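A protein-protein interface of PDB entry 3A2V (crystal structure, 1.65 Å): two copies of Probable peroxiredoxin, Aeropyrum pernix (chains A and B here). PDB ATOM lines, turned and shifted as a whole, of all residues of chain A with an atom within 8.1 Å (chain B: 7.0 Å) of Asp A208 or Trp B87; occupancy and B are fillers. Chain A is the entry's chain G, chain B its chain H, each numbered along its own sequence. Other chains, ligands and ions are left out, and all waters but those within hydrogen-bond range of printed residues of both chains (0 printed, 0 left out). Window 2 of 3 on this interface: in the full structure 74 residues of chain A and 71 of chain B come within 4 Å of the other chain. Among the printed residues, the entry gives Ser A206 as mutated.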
ATOM      1  N   ILE A 179     -23.493  -4.198  29.162  1.00  0.00           N
ATOM      2  CA  ILE A 179     -22.233  -4.923  29.347  1.00  0.00           C
ATOM      3  C   ILE A 179     -21.556  -4.483  30.636  1.00  0.00           C
ATOM      4  O   ILE A 179     -21.171  -5.341  31.446  1.00  0.00           O
ATOM      5  CB  ILE A 179     -21.259  -4.766  28.159  1.00  0.00           C
ATOM      6  CG1 ILE A 179     -21.919  -5.277  26.877  1.00  0.00           C
ATOM      7  CG2 ILE A 179     -19.955  -5.579  28.436  1.00  0.00           C
ATOM      8  CD1 ILE A 179     -21.114  -4.994  25.584  1.00  0.00           C
ATOM      9  N   PRO A 188      -9.379   3.379  23.581  1.00  0.00           N
ATOM     10  CA  PRO A 188      -8.506   2.217  23.328  1.00  0.00           C
ATOM     11  C   PRO A 188      -7.086   2.613  22.926  1.00  0.00           C
ATOM     12  O   PRO A 188      -6.867   3.704  22.402  1.00  0.00           O
ATOM     13  CB  PRO A 188      -9.223   1.458  22.205  1.00  0.00           C
ATOM     14  CG  PRO A 188     -10.024   2.545  21.458  1.00  0.00           C
ATOM     15  CD  PRO A 188     -10.466   3.486  22.581  1.00  0.00           C
ATOM     16  N   PRO A 189      -6.113   1.723  23.177  1.00  0.00           N
ATOM     17  CA  PRO A 189      -4.743   2.033  22.745  1.00  0.00           C
ATOM     18  C   PRO A 189      -4.671   2.096  21.219  1.00  0.00           C
ATOM     19  O   PRO A 189      -5.437   1.401  20.543  1.00  0.00           O
ATOM     20  CB  PRO A 189      -3.941   0.833  23.242  1.00  0.00           C
ATOM     21  CG  PRO A 189      -4.790   0.227  24.367  1.00  0.00           C
ATOM     22  CD  PRO A 189      -6.208   0.410  23.831  1.00  0.00           C
ATOM     23  N   ALA A 195      -0.821  -0.935  23.725  1.00  0.00           N
ATOM     24  CA  ALA A 195      -1.739  -2.049  23.958  1.00  0.00           C
ATOM     25  C   ALA A 195      -1.116  -3.050  24.952  1.00  0.00           C
ATOM     26  O   ALA A 195      -1.763  -3.474  25.909  1.00  0.00           O
ATOM     27  CB  ALA A 195      -2.080  -2.735  22.667  1.00  0.00           C
ATOM     28  N   ARG A 198      -0.725  -1.459  28.589  1.00  0.00           N
ATOM     29  CA  ARG A 198      -2.000  -1.412  29.299  1.00  0.00           C
ATOM     30  C   ARG A 198      -2.353  -2.766  29.884  1.00  0.00           C
ATOM     31  O   ARG A 198      -2.812  -2.851  31.028  1.00  0.00           O
ATOM     32  CB  ARG A 198      -3.139  -0.923  28.403  1.00  0.00           C
ATOM     33  CG  ARG A 198      -4.418  -0.763  29.183  1.00  0.00           C
ATOM     34  CD  ARG A 198      -5.412   0.101  28.482  1.00  0.00           C
ATOM     35  NE  ARG A 198      -4.892   1.443  28.284  1.00  0.00           N
ATOM     36  CZ  ARG A 198      -5.457   2.358  27.498  1.00  0.00           C
ATOM     37  NH1 ARG A 198      -6.579   2.076  26.825  1.00  0.00           N
ATOM     38  NH2 ARG A 198      -4.890   3.549  27.381  1.00  0.00           N
ATOM     39  N   MET A 199      -2.135  -3.822  29.105  1.00  0.00           N
ATOM     40  CA  MET A 199      -2.475  -5.176  29.542  1.00  0.00           C
ATOM     41  C   MET A 199      -1.585  -5.671  30.677  1.00  0.00           C
ATOM     42  O   MET A 199      -2.050  -6.384  31.577  1.00  0.00           O
ATOM     43  CB  MET A 199      -2.445  -6.157  28.372  1.00  0.00           C
ATOM     44  CG  MET A 199      -3.654  -6.056  27.466  1.00  0.00           C
ATOM     45  SD  MET A 199      -5.260  -5.926  28.315  1.00  0.00           S
ATOM     46  CE  MET A 199      -5.356  -4.173  28.588  1.00  0.00           C
ATOM     47  N   TYR A 204      -6.983  -1.963  34.829  1.00  0.00           N
ATOM     48  CA  TYR A 204      -8.424  -1.827  34.550  1.00  0.00           C
ATOM     49  C   TYR A 204      -9.117  -3.170  34.427  1.00  0.00           C
ATOM     50  O   TYR A 204      -8.478  -4.171  34.086  1.00  0.00           O
ATOM     51  CB  TYR A 204      -8.634  -1.077  33.221  1.00  0.00           C
ATOM     52  CG  TYR A 204      -7.965   0.273  33.114  1.00  0.00           C
ATOM     53  CD1 TYR A 204      -6.863   0.469  32.269  1.00  0.00           C
ATOM     54  CD2 TYR A 204      -8.440   1.379  33.855  1.00  0.00           C
ATOM     55  CE1 TYR A 204      -6.255   1.733  32.160  1.00  0.00           C
ATOM     56  CE2 TYR A 204      -7.848   2.621  33.748  1.00  0.00           C
ATOM     57  CZ  TYR A 204      -6.755   2.803  32.911  1.00  0.00           C
ATOM     58  OH  TYR A 204      -6.187   4.044  32.834  1.00  0.00           O
ATOM     59  N   ARG A 205     -10.431  -3.181  34.663  1.00  0.00           N
ATOM     60  CA  ARG A 205     -11.301  -4.260  34.214  1.00  0.00           C
ATOM     61  C   ARG A 205     -11.209  -4.282  32.679  1.00  0.00           C
ATOM     62  O   ARG A 205     -10.991  -3.242  32.063  1.00  0.00           O
ATOM     63  CB  ARG A 205     -12.752  -4.033  34.678  1.00  0.00           C
ATOM     64  CG  ARG A 205     -12.983  -4.465  36.166  1.00  0.00           C
ATOM     65  CD  ARG A 205     -14.196  -3.812  36.848  1.00  0.00           C
ATOM     66  NE  ARG A 205     -13.852  -2.468  37.313  1.00  0.00           N
ATOM     67  CZ  ARG A 205     -14.638  -1.661  38.029  1.00  0.00           C
ATOM     68  NH1 ARG A 205     -15.856  -2.046  38.406  1.00  0.00           N
ATOM     69  NH2 ARG A 205     -14.185  -0.462  38.382  1.00  0.00           N
ATOM     70  N   SER A 206     -11.335  -5.453  32.084  1.00  0.00           N
ATOM     71  CA  SER A 206     -10.942  -5.600  30.670  1.00  0.00           C
ATOM     72  C   SER A 206     -11.571  -6.811  30.035  1.00  0.00           C
ATOM     73  O   SER A 206     -11.611  -7.878  30.647  1.00  0.00           O
ATOM     74  CB  SER A 206      -9.403  -5.703  30.597  1.00  0.00           C
ATOM     75  OG  SER A 206      -8.931  -5.818  29.275  1.00  0.00           O
ATOM     76  N   LEU A 207     -12.086  -6.658  28.813  1.00  0.00           N
ATOM     77  CA  LEU A 207     -12.514  -7.811  28.031  1.00  0.00           C
ATOM     78  C   LEU A 207     -11.483  -8.172  26.948  1.00  0.00           C
ATOM     79  O   LEU A 207     -11.492  -9.300  26.439  1.00  0.00           O
ATOM     80  CB  LEU A 207     -13.867  -7.518  27.385  1.00  0.00           C
ATOM     81  CG  LEU A 207     -15.195  -7.835  28.085  1.00  0.00           C
ATOM     82  CD1 LEU A 207     -15.073  -7.956  29.542  1.00  0.00           C
ATOM     83  CD2 LEU A 207     -16.290  -6.837  27.698  1.00  0.00           C
ATOM     84  N   ASP A 208     -10.654  -7.190  26.602  1.00  0.00           N
ATOM     85  CA  ASP A 208      -9.524  -7.319  25.647  1.00  0.00           C
ATOM     86  C   ASP A 208      -8.704  -6.030  25.746  1.00  0.00           C
ATOM     87  O   ASP A 208      -9.141  -5.064  26.380  1.00  0.00           O
ATOM     88  CB  ASP A 208     -10.037  -7.597  24.210  1.00  0.00           C
ATOM     89  CG  ASP A 208      -8.981  -8.292  23.307  1.00  0.00           C
ATOM     90  OD1 ASP A 208      -7.853  -8.569  23.784  1.00  0.00           O
ATOM     91  OD2 ASP A 208      -9.293  -8.566  22.114  1.00  0.00           O
ATOM     92  N   TRP A 209      -7.509  -5.992  25.150  1.00  0.00           N
ATOM     93  CA  TRP A 209      -6.639  -4.816  25.264  1.00  0.00           C
ATOM     94  C   TRP A 209      -7.360  -3.553  24.786  1.00  0.00           C
ATOM     95  O   TRP A 209      -7.044  -2.454  25.215  1.00  0.00           O
ATOM     96  CB  TRP A 209      -5.286  -4.977  24.522  1.00  0.00           C
ATOM     97  CG  TRP A 209      -5.434  -5.248  23.065  1.00  0.00           C
ATOM     98  CD1 TRP A 209      -5.494  -6.460  22.469  1.00  0.00           C
ATOM     99  CD2 TRP A 209      -5.592  -4.270  22.023  1.00  0.00           C
ATOM    100  NE1 TRP A 209      -5.665  -6.319  21.112  1.00  0.00           N
ATOM    101  CE2 TRP A 209      -5.734  -4.986  20.810  1.00  0.00           C
ATOM    102  CE3 TRP A 209      -5.603  -2.862  21.996  1.00  0.00           C
ATOM    103  CZ2 TRP A 209      -5.914  -4.339  19.571  1.00  0.00           C
ATOM    104  CZ3 TRP A 209      -5.793  -2.203  20.741  1.00  0.00           C
ATOM    105  CH2 TRP A 209      -5.926  -2.957  19.559  1.00  0.00           C
ATOM    106  N   TRP A 210      -8.325  -3.729  23.887  1.00  0.00           N
ATOM    107  CA  TRP A 210      -9.017  -2.561  23.314  1.00  0.00           C
ATOM    108  C   TRP A 210     -10.315  -2.247  24.058  1.00  0.00           C
ATOM    109  O   TRP A 210     -10.969  -1.256  23.758  1.00  0.00           O
ATOM    110  CB  TRP A 210      -9.325  -2.796  21.829  1.00  0.00           C
ATOM    111  CG  TRP A 210     -10.017  -4.068  21.566  1.00  0.00           C
ATOM    112  CD1 TRP A 210      -9.443  -5.272  21.288  1.00  0.00           C
ATOM    113  CD2 TRP A 210     -11.435  -4.282  21.514  1.00  0.00           C
ATOM    114  NE1 TRP A 210     -10.402  -6.226  21.091  1.00  0.00           N
ATOM    115  CE2 TRP A 210     -11.641  -5.647  21.219  1.00  0.00           C
ATOM    116  CE3 TRP A 210     -12.546  -3.456  21.711  1.00  0.00           C
ATOM    117  CZ2 TRP A 210     -12.919  -6.214  21.105  1.00  0.00           C
ATOM    118  CZ3 TRP A 210     -13.826  -4.015  21.586  1.00  0.00           C
ATOM    119  CH2 TRP A 210     -14.002  -5.368  21.289  1.00  0.00           C
ATOM    120  N   PHE A 211     -10.642  -3.056  25.067  1.00  0.00           N
ATOM    121  CA  PHE A 211     -11.876  -2.892  25.829  1.00  0.00           C
ATOM    122  C   PHE A 211     -11.567  -2.939  27.336  1.00  0.00           C
ATOM    123  O   PHE A 211     -11.720  -3.990  27.977  1.00  0.00           O
ATOM    124  CB  PHE A 211     -12.916  -3.954  25.431  1.00  0.00           C
ATOM    125  CG  PHE A 211     -14.377  -3.595  25.816  1.00  0.00           C
ATOM    126  CD1 PHE A 211     -15.433  -4.111  25.086  1.00  0.00           C
ATOM    127  CD2 PHE A 211     -14.668  -2.727  26.893  1.00  0.00           C
ATOM    128  CE1 PHE A 211     -16.795  -3.813  25.411  1.00  0.00           C
ATOM    129  CE2 PHE A 211     -16.021  -2.402  27.239  1.00  0.00           C
ATOM    130  CZ  PHE A 211     -17.090  -2.974  26.496  1.00  0.00           C
ATOM    131  N   CYS A 212     -11.108  -1.807  27.847  1.00  0.00           N
ATOM    132  CA  CYS A 212     -10.842  -1.636  29.269  1.00  0.00           C
ATOM    133  C   CYS A 212     -11.777  -0.580  29.817  1.00  0.00           C
ATOM    134  O   CYS A 212     -12.091   0.402  29.124  1.00  0.00           O
ATOM    135  CB  CYS A 212      -9.429  -1.150  29.428  1.00  0.00           C
ATOM    136  SG  CYS A 212      -8.203  -2.488  29.133  1.00  0.00           S
ATOM    137  N   TRP A 213     -12.225  -0.762  31.058  1.00  0.00           N
ATOM    138  CA  TRP A 213     -13.134   0.212  31.654  1.00  0.00           C
ATOM    139  C   TRP A 213     -12.973   0.263  33.154  1.00  0.00           C
ATOM    140  O   TRP A 213     -12.320  -0.593  33.745  1.00  0.00           O
ATOM    141  CB  TRP A 213     -14.589  -0.107  31.300  1.00  0.00           C
ATOM    142  CG  TRP A 213     -15.256  -1.098  32.209  1.00  0.00           C
ATOM    143  CD1 TRP A 213     -15.936  -0.828  33.376  1.00  0.00           C
ATOM    144  CD2 TRP A 213     -15.320  -2.510  32.025  1.00  0.00           C
ATOM    145  NE1 TRP A 213     -16.420  -1.996  33.919  1.00  0.00           N
ATOM    146  CE2 TRP A 213     -16.056  -3.042  33.111  1.00  0.00           C
ATOM    147  CE3 TRP A 213     -14.835  -3.382  31.043  1.00  0.00           C
ATOM    148  CZ2 TRP A 213     -16.307  -4.408  33.246  1.00  0.00           C
ATOM    149  CZ3 TRP A 213     -15.092  -4.747  31.182  1.00  0.00           C
ATOM    150  CH2 TRP A 213     -15.823  -5.241  32.265  1.00  0.00           C
ATOM    151  N   PHE B  45     -13.651  -3.558  16.624  1.00  0.00           N
ATOM    152  CA  PHE B  45     -12.636  -3.768  17.683  1.00  0.00           C
ATOM    153  C   PHE B  45     -12.339  -2.489  18.476  1.00  0.00           C
ATOM    154  O   PHE B  45     -11.200  -2.215  18.926  1.00  0.00           O
ATOM    155  CB  PHE B  45     -11.382  -4.426  17.106  1.00  0.00           C
ATOM    156  CG  PHE B  45     -11.605  -5.845  16.710  1.00  0.00           C
ATOM    157  CD1 PHE B  45     -11.714  -6.191  15.367  1.00  0.00           C
ATOM    158  CD2 PHE B  45     -11.748  -6.852  17.678  1.00  0.00           C
ATOM    159  CE1 PHE B  45     -11.964  -7.511  15.001  1.00  0.00           C
ATOM    160  CE2 PHE B  45     -11.990  -8.175  17.309  1.00  0.00           C
ATOM    161  CZ  PHE B  45     -12.067  -8.501  15.978  1.00  0.00           C
ATOM    162  N   THR B  50     -18.656  -1.631  20.204  1.00  0.00           N
ATOM    163  CA  THR B  50     -19.040  -2.951  20.648  1.00  0.00           C
ATOM    164  C   THR B  50     -20.291  -2.884  21.548  1.00  0.00           C
ATOM    165  O   THR B  50     -21.247  -3.669  21.352  1.00  0.00           O
ATOM    166  CB  THR B  50     -17.822  -3.623  21.341  1.00  0.00           C
ATOM    167  OG1 THR B  50     -16.799  -3.752  20.364  1.00  0.00           O
ATOM    168  CG2 THR B  50     -18.163  -5.000  21.815  1.00  0.00           C
ATOM    169  N   HIS B  81     -15.281  -7.236   9.899  1.00  0.00           N
ATOM    170  CA  HIS B  81     -16.635  -7.397  10.421  1.00  0.00           C
ATOM    171  C   HIS B  81     -16.915  -8.814  10.916  1.00  0.00           C
ATOM    172  O   HIS B  81     -17.527  -9.023  11.975  1.00  0.00           O
ATOM    173  CB  HIS B  81     -17.677  -7.038   9.364  1.00  0.00           C
ATOM    174  CG  HIS B  81     -17.703  -5.585   8.982  1.00  0.00           C
ATOM    175  ND1 HIS B  81     -17.039  -4.600   9.684  1.00  0.00           N
ATOM    176  CD2 HIS B  81     -18.387  -4.948   7.995  1.00  0.00           C
ATOM    177  CE1 HIS B  81     -17.276  -3.425   9.119  1.00  0.00           C
ATOM    178  NE2 HIS B  81     -18.103  -3.608   8.107  1.00  0.00           N
ATOM    179  N   ILE B  82     -16.498  -9.809  10.126  1.00  0.00           N
ATOM    180  CA  ILE B  82     -16.773 -11.180  10.494  1.00  0.00           C
ATOM    181  C   ILE B  82     -15.957 -11.569  11.745  1.00  0.00           C
ATOM    182  O   ILE B  82     -16.502 -12.187  12.665  1.00  0.00           O
ATOM    183  CB  ILE B  82     -16.498 -12.136   9.308  1.00  0.00           C
ATOM    184  CG1 ILE B  82     -17.469 -11.799   8.147  1.00  0.00           C
ATOM    185  CG2 ILE B  82     -16.739 -13.563   9.747  1.00  0.00           C
ATOM    186  CD1 ILE B  82     -16.994 -12.373   6.789  1.00  0.00           C
ATOM    187  N   LYS B  83     -14.698 -11.146  11.806  1.00  0.00           N
ATOM    188  CA  LYS B  83     -13.845 -11.429  12.988  1.00  0.00           C
ATOM    189  C   LYS B  83     -14.413 -10.760  14.260  1.00  0.00           C
ATOM    190  O   LYS B  83     -14.368 -11.322  15.376  1.00  0.00           O
ATOM    191  CB  LYS B  83     -12.414 -10.910  12.782  1.00  0.00           C
ATOM    192  CG  LYS B  83     -11.498 -11.747  11.854  1.00  0.00           C
ATOM    193  CD  LYS B  83     -11.487 -13.260  12.146  1.00  0.00           C
ATOM    194  CE  LYS B  83     -10.719 -13.643  13.409  1.00  0.00           C
ATOM    195  NZ  LYS B  83     -11.021 -15.095  13.719  1.00  0.00           N
ATOM    196  N   TRP B  84     -14.953  -9.555  14.074  1.00  0.00           N
ATOM    197  CA  TRP B  84     -15.464  -8.799  15.221  1.00  0.00           C
ATOM    198  C   TRP B  84     -16.714  -9.455  15.737  1.00  0.00           C
ATOM    199  O   TRP B  84     -16.885  -9.608  16.949  1.00  0.00           O
ATOM    200  CB  TRP B  84     -15.734  -7.366  14.798  1.00  0.00           C
ATOM    201  CG  TRP B  84     -16.095  -6.414  15.900  1.00  0.00           C
ATOM    202  CD1 TRP B  84     -15.572  -6.348  17.177  1.00  0.00           C
ATOM    203  CD2 TRP B  84     -16.996  -5.314  15.782  1.00  0.00           C
ATOM    204  NE1 TRP B  84     -16.114  -5.268  17.854  1.00  0.00           N
ATOM    205  CE2 TRP B  84     -17.010  -4.642  17.024  1.00  0.00           C
ATOM    206  CE3 TRP B  84     -17.846  -4.865  14.754  1.00  0.00           C
ATOM    207  CZ2 TRP B  84     -17.808  -3.516  17.250  1.00  0.00           C
ATOM    208  CZ3 TRP B  84     -18.639  -3.742  14.986  1.00  0.00           C
ATOM    209  CH2 TRP B  84     -18.621  -3.091  16.215  1.00  0.00           C
ATOM    210  N   LYS B  85     -17.611  -9.833  14.832  1.00  0.00           N
ATOM    211  CA  LYS B  85     -18.798 -10.583  15.210  1.00  0.00           C
ATOM    212  C   LYS B  85     -18.476 -11.882  15.934  1.00  0.00           C
ATOM    213  O   LYS B  85     -19.113 -12.221  16.927  1.00  0.00           O
ATOM    214  CB  LYS B  85     -19.710 -10.827  14.010  1.00  0.00           C
ATOM    215  CG  LYS B  85     -20.440  -9.560  13.555  1.00  0.00           C
ATOM    216  CD  LYS B  85     -21.267  -9.858  12.287  1.00  0.00           C
ATOM    217  CE  LYS B  85     -22.424  -8.833  12.139  1.00  0.00           C
ATOM    218  NZ  LYS B  85     -22.992  -8.933  10.772  1.00  0.00           N
ATOM    219  N   GLU B  86     -17.478 -12.602  15.430  1.00  0.00           N
ATOM    220  CA  GLU B  86     -16.967 -13.783  16.112  1.00  0.00           C
ATOM    221  C   GLU B  86     -16.547 -13.431  17.549  1.00  0.00           C
ATOM    222  O   GLU B  86     -16.861 -14.161  18.478  1.00  0.00           O
ATOM    223  CB  GLU B  86     -15.742 -14.296  15.363  1.00  0.00           C
ATOM    224  CG  GLU B  86     -15.982 -15.286  14.291  1.00  0.00           C
ATOM    225  CD  GLU B  86     -14.663 -15.911  13.830  1.00  0.00           C
ATOM    226  OE1 GLU B  86     -13.747 -15.162  13.426  1.00  0.00           O
ATOM    227  OE2 GLU B  86     -14.524 -17.145  13.921  1.00  0.00           O
ATOM    228  N   TRP B  87     -15.822 -12.331  17.714  1.00  0.00           N
ATOM    229  CA  TRP B  87     -15.303 -11.921  19.019  1.00  0.00           C
ATOM    230  C   TRP B  87     -16.456 -11.637  19.994  1.00  0.00           C
ATOM    231  O   TRP B  87     -16.490 -12.098  21.162  1.00  0.00           O
ATOM    232  CB  TRP B  87     -14.362 -10.730  18.880  1.00  0.00           C
ATOM    233  CG  TRP B  87     -13.710 -10.350  20.198  1.00  0.00           C
ATOM    234  CD1 TRP B  87     -12.451 -10.672  20.609  1.00  0.00           C
ATOM    235  CD2 TRP B  87     -14.310  -9.603  21.268  1.00  0.00           C
ATOM    236  NE1 TRP B  87     -12.228 -10.179  21.878  1.00  0.00           N
ATOM    237  CE2 TRP B  87     -13.348  -9.511  22.301  1.00  0.00           C
ATOM    238  CE3 TRP B  87     -15.561  -8.993  21.451  1.00  0.00           C
ATOM    239  CZ2 TRP B  87     -13.600  -8.841  23.515  1.00  0.00           C
ATOM    240  CZ3 TRP B  87     -15.818  -8.319  22.678  1.00  0.00           C
ATOM    241  CH2 TRP B  87     -14.832  -8.250  23.678  1.00  0.00           C
ATOM    242  N   ILE B  88     -17.427 -10.877  19.509  1.00  0.00           N
ATOM    243  CA  ILE B  88     -18.570 -10.532  20.344  1.00  0.00           C
ATOM    244  C   ILE B  88     -19.323 -11.785  20.778  1.00  0.00           C
ATOM    245  O   ILE B  88     -19.678 -11.914  21.953  1.00  0.00           O
ATOM    246  CB  ILE B  88     -19.493  -9.525  19.617  1.00  0.00           C
ATOM    247  CG1 ILE B  88     -18.748  -8.186  19.433  1.00  0.00           C
ATOM    248  CG2 ILE B  88     -20.807  -9.328  20.391  1.00  0.00           C
ATOM    249  CD1 ILE B  88     -19.492  -7.164  18.478  1.00  0.00           C
ATOM    250  N   GLU B  89     -19.558 -12.719  19.849  1.00  0.00           N
ATOM    251  CA  GLU B  89     -20.267 -13.938  20.202  1.00  0.00           C
ATOM    252  C   GLU B  89     -19.474 -14.775  21.217  1.00  0.00           C
ATOM    253  O   GLU B  89     -20.044 -15.258  22.200  1.00  0.00           O
ATOM    254  CB  GLU B  89     -20.584 -14.772  18.976  1.00  0.00           C
ATOM    255  CG  GLU B  89     -21.419 -15.991  19.318  1.00  0.00           C
ATOM    256  CD  GLU B  89     -21.871 -16.742  18.095  1.00  0.00           C
ATOM    257  OE1 GLU B  89     -21.539 -17.940  17.978  1.00  0.00           O
ATOM    258  OE2 GLU B  89     -22.536 -16.138  17.238  1.00  0.00           O
ATOM    259  N   ARG B  90     -18.176 -14.909  20.991  1.00  0.00           N
ATOM    260  CA  ARG B  90     -17.304 -15.699  21.873  1.00  0.00           C
ATOM    261  C   ARG B  90     -17.147 -15.086  23.265  1.00  0.00           C
ATOM    262  O   ARG B  90     -17.218 -15.812  24.263  1.00  0.00           O
ATOM    263  CB  ARG B  90     -15.941 -15.902  21.217  1.00  0.00           C
ATOM    264  CG  ARG B  90     -14.917 -16.695  22.064  1.00  0.00           C
ATOM    265  CD  ARG B  90     -14.213 -17.778  21.216  1.00  0.00           C
ATOM    266  NE  ARG B  90     -13.602 -17.255  19.983  1.00  0.00           N
ATOM    267  CZ  ARG B  90     -14.010 -17.537  18.737  1.00  0.00           C
ATOM    268  NH1 ARG B  90     -15.053 -18.345  18.513  1.00  0.00           N
ATOM    269  NH2 ARG B  90     -13.370 -17.002  17.704  1.00  0.00           N
ATOM    270  N   HIS B  91     -16.958 -13.764  23.342  1.00  0.00           N
ATOM    271  CA  HIS B  91     -16.583 -13.102  24.597  1.00  0.00           C
ATOM    272  C   HIS B  91     -17.744 -12.475  25.374  1.00  0.00           C
ATOM    273  O   HIS B  91     -17.712 -12.444  26.611  1.00  0.00           O
ATOM    274  CB  HIS B  91     -15.451 -12.087  24.377  1.00  0.00           C
ATOM    275  CG  HIS B  91     -14.177 -12.726  23.917  1.00  0.00           C
ATOM    276  ND1 HIS B  91     -13.221 -13.201  24.790  1.00  0.00           N
ATOM    277  CD2 HIS B  91     -13.740 -13.036  22.671  1.00  0.00           C
ATOM    278  CE1 HIS B  91     -12.235 -13.751  24.101  1.00  0.00           C
ATOM    279  NE2 HIS B  91     -12.527 -13.669  22.813  1.00  0.00           N
ATOM    280  N   ILE B  92     -18.750 -11.983  24.662  1.00  0.00           N
ATOM    281  CA  ILE B  92     -19.931 -11.385  25.285  1.00  0.00           C
ATOM    282  C   ILE B  92     -21.108 -12.353  25.279  1.00  0.00           C
ATOM    283  O   ILE B  92     -22.036 -12.223  26.070  1.00  0.00           O
ATOM    284  CB  ILE B  92     -20.362 -10.065  24.544  1.00  0.00           C
ATOM    285  CG1 ILE B  92     -19.180  -9.127  24.284  1.00  0.00           C
ATOM    286  CG2 ILE B  92     -21.470  -9.316  25.317  1.00  0.00           C
ATOM    287  CD1 ILE B  92     -18.437  -8.633  25.515  1.00  0.00           C
ATOM    288  N   GLY B  93     -21.073 -13.324  24.378  1.00  0.00           N
ATOM    289  CA  GLY B  93     -22.132 -14.309  24.269  1.00  0.00           C
ATOM    290  C   GLY B  93     -23.362 -13.784  23.555  1.00  0.00           C
ATOM    291  O   GLY B  93     -24.471 -14.277  23.765  1.00  0.00           O
ATOM    292  N   VAL B  94     -23.162 -12.768  22.711  1.00  0.00           N
ATOM    293  CA  VAL B  94     -24.253 -12.166  21.950  1.00  0.00           C
ATOM    294  C   VAL B  94     -23.965 -12.319  20.454  1.00  0.00           C
ATOM    295  O   VAL B  94     -22.877 -11.957  20.000  1.00  0.00           O
ATOM    296  CB  VAL B  94     -24.414 -10.667  22.332  1.00  0.00           C
ATOM    297  CG1 VAL B  94     -25.394  -9.948  21.388  1.00  0.00           C
ATOM    298  CG2 VAL B  94     -24.860 -10.532  23.794  1.00  0.00           C
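The indole nitrogen (NE1) of Trp B87 is in hydrogen-bond range of the side-chain carboxylate (OD2) of Asp A208 (3.4 Å).
OG of Ser A206 is in hydrogen-bond range of O of Asp A208, 3.0 Å away. The indole nitrogen (NE1) of Trp B84 is in hydrogen-bond range of the side-chain hydroxyl (OG1) of Thr B50 (3.0 Å). The indole nitrogen (NE1) of Trp A210 lies within hydrogen-bond range of the side-chain carboxylate (OD2) of Asp A208 (2.8 Å).
Leu A207 touches Trp B87. Ile B92 touches Leu A207 (CD1 to CD2, 3.5 Å). Trp A210 touches Phe B45 (CD2 to O, 3.3 Å). Thr B50 touches Trp A210. Trp A210 touches Trp B87 (CZ2 to CE2, 3.5 Å).
Asp A208 touches one residue of chain B. Of chain A, only Leu A207, Asp A208 and Trp A210 come within 4 Å of Trp B87. Printed residues of chain A within 4 Å of Thr B50: Trp A210. Of the printed residues of chain B, Trp A210 touches Phe B45, Thr B50 and Trp B87. Trp B84 touches none of the printed residues of chain A. The nearest printed residue of chain A that does not touch Ile B92 is Ile A179 (4.3 Å).
Of the 16 printed residues of chain B, 4 touch a printed residue of chain A. Hydrophobic or aromatic side chains of chain B that line the printed part of chain A: Phe B45, Trp B87 and Ile B92. Of the 16 printed residues of chain A, 3 touch a printed residue of chain B. Hydrophobic or aromatic side chains of chain A within 4 Å of the printed part of chain B: Leu A207 and Trp A210. Among the printed residues, no Asp or Glu carboxylate lies within 4 Å of a Lys or Arg side-chain nitrogen of the other chain.
No position is printed for both chains.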
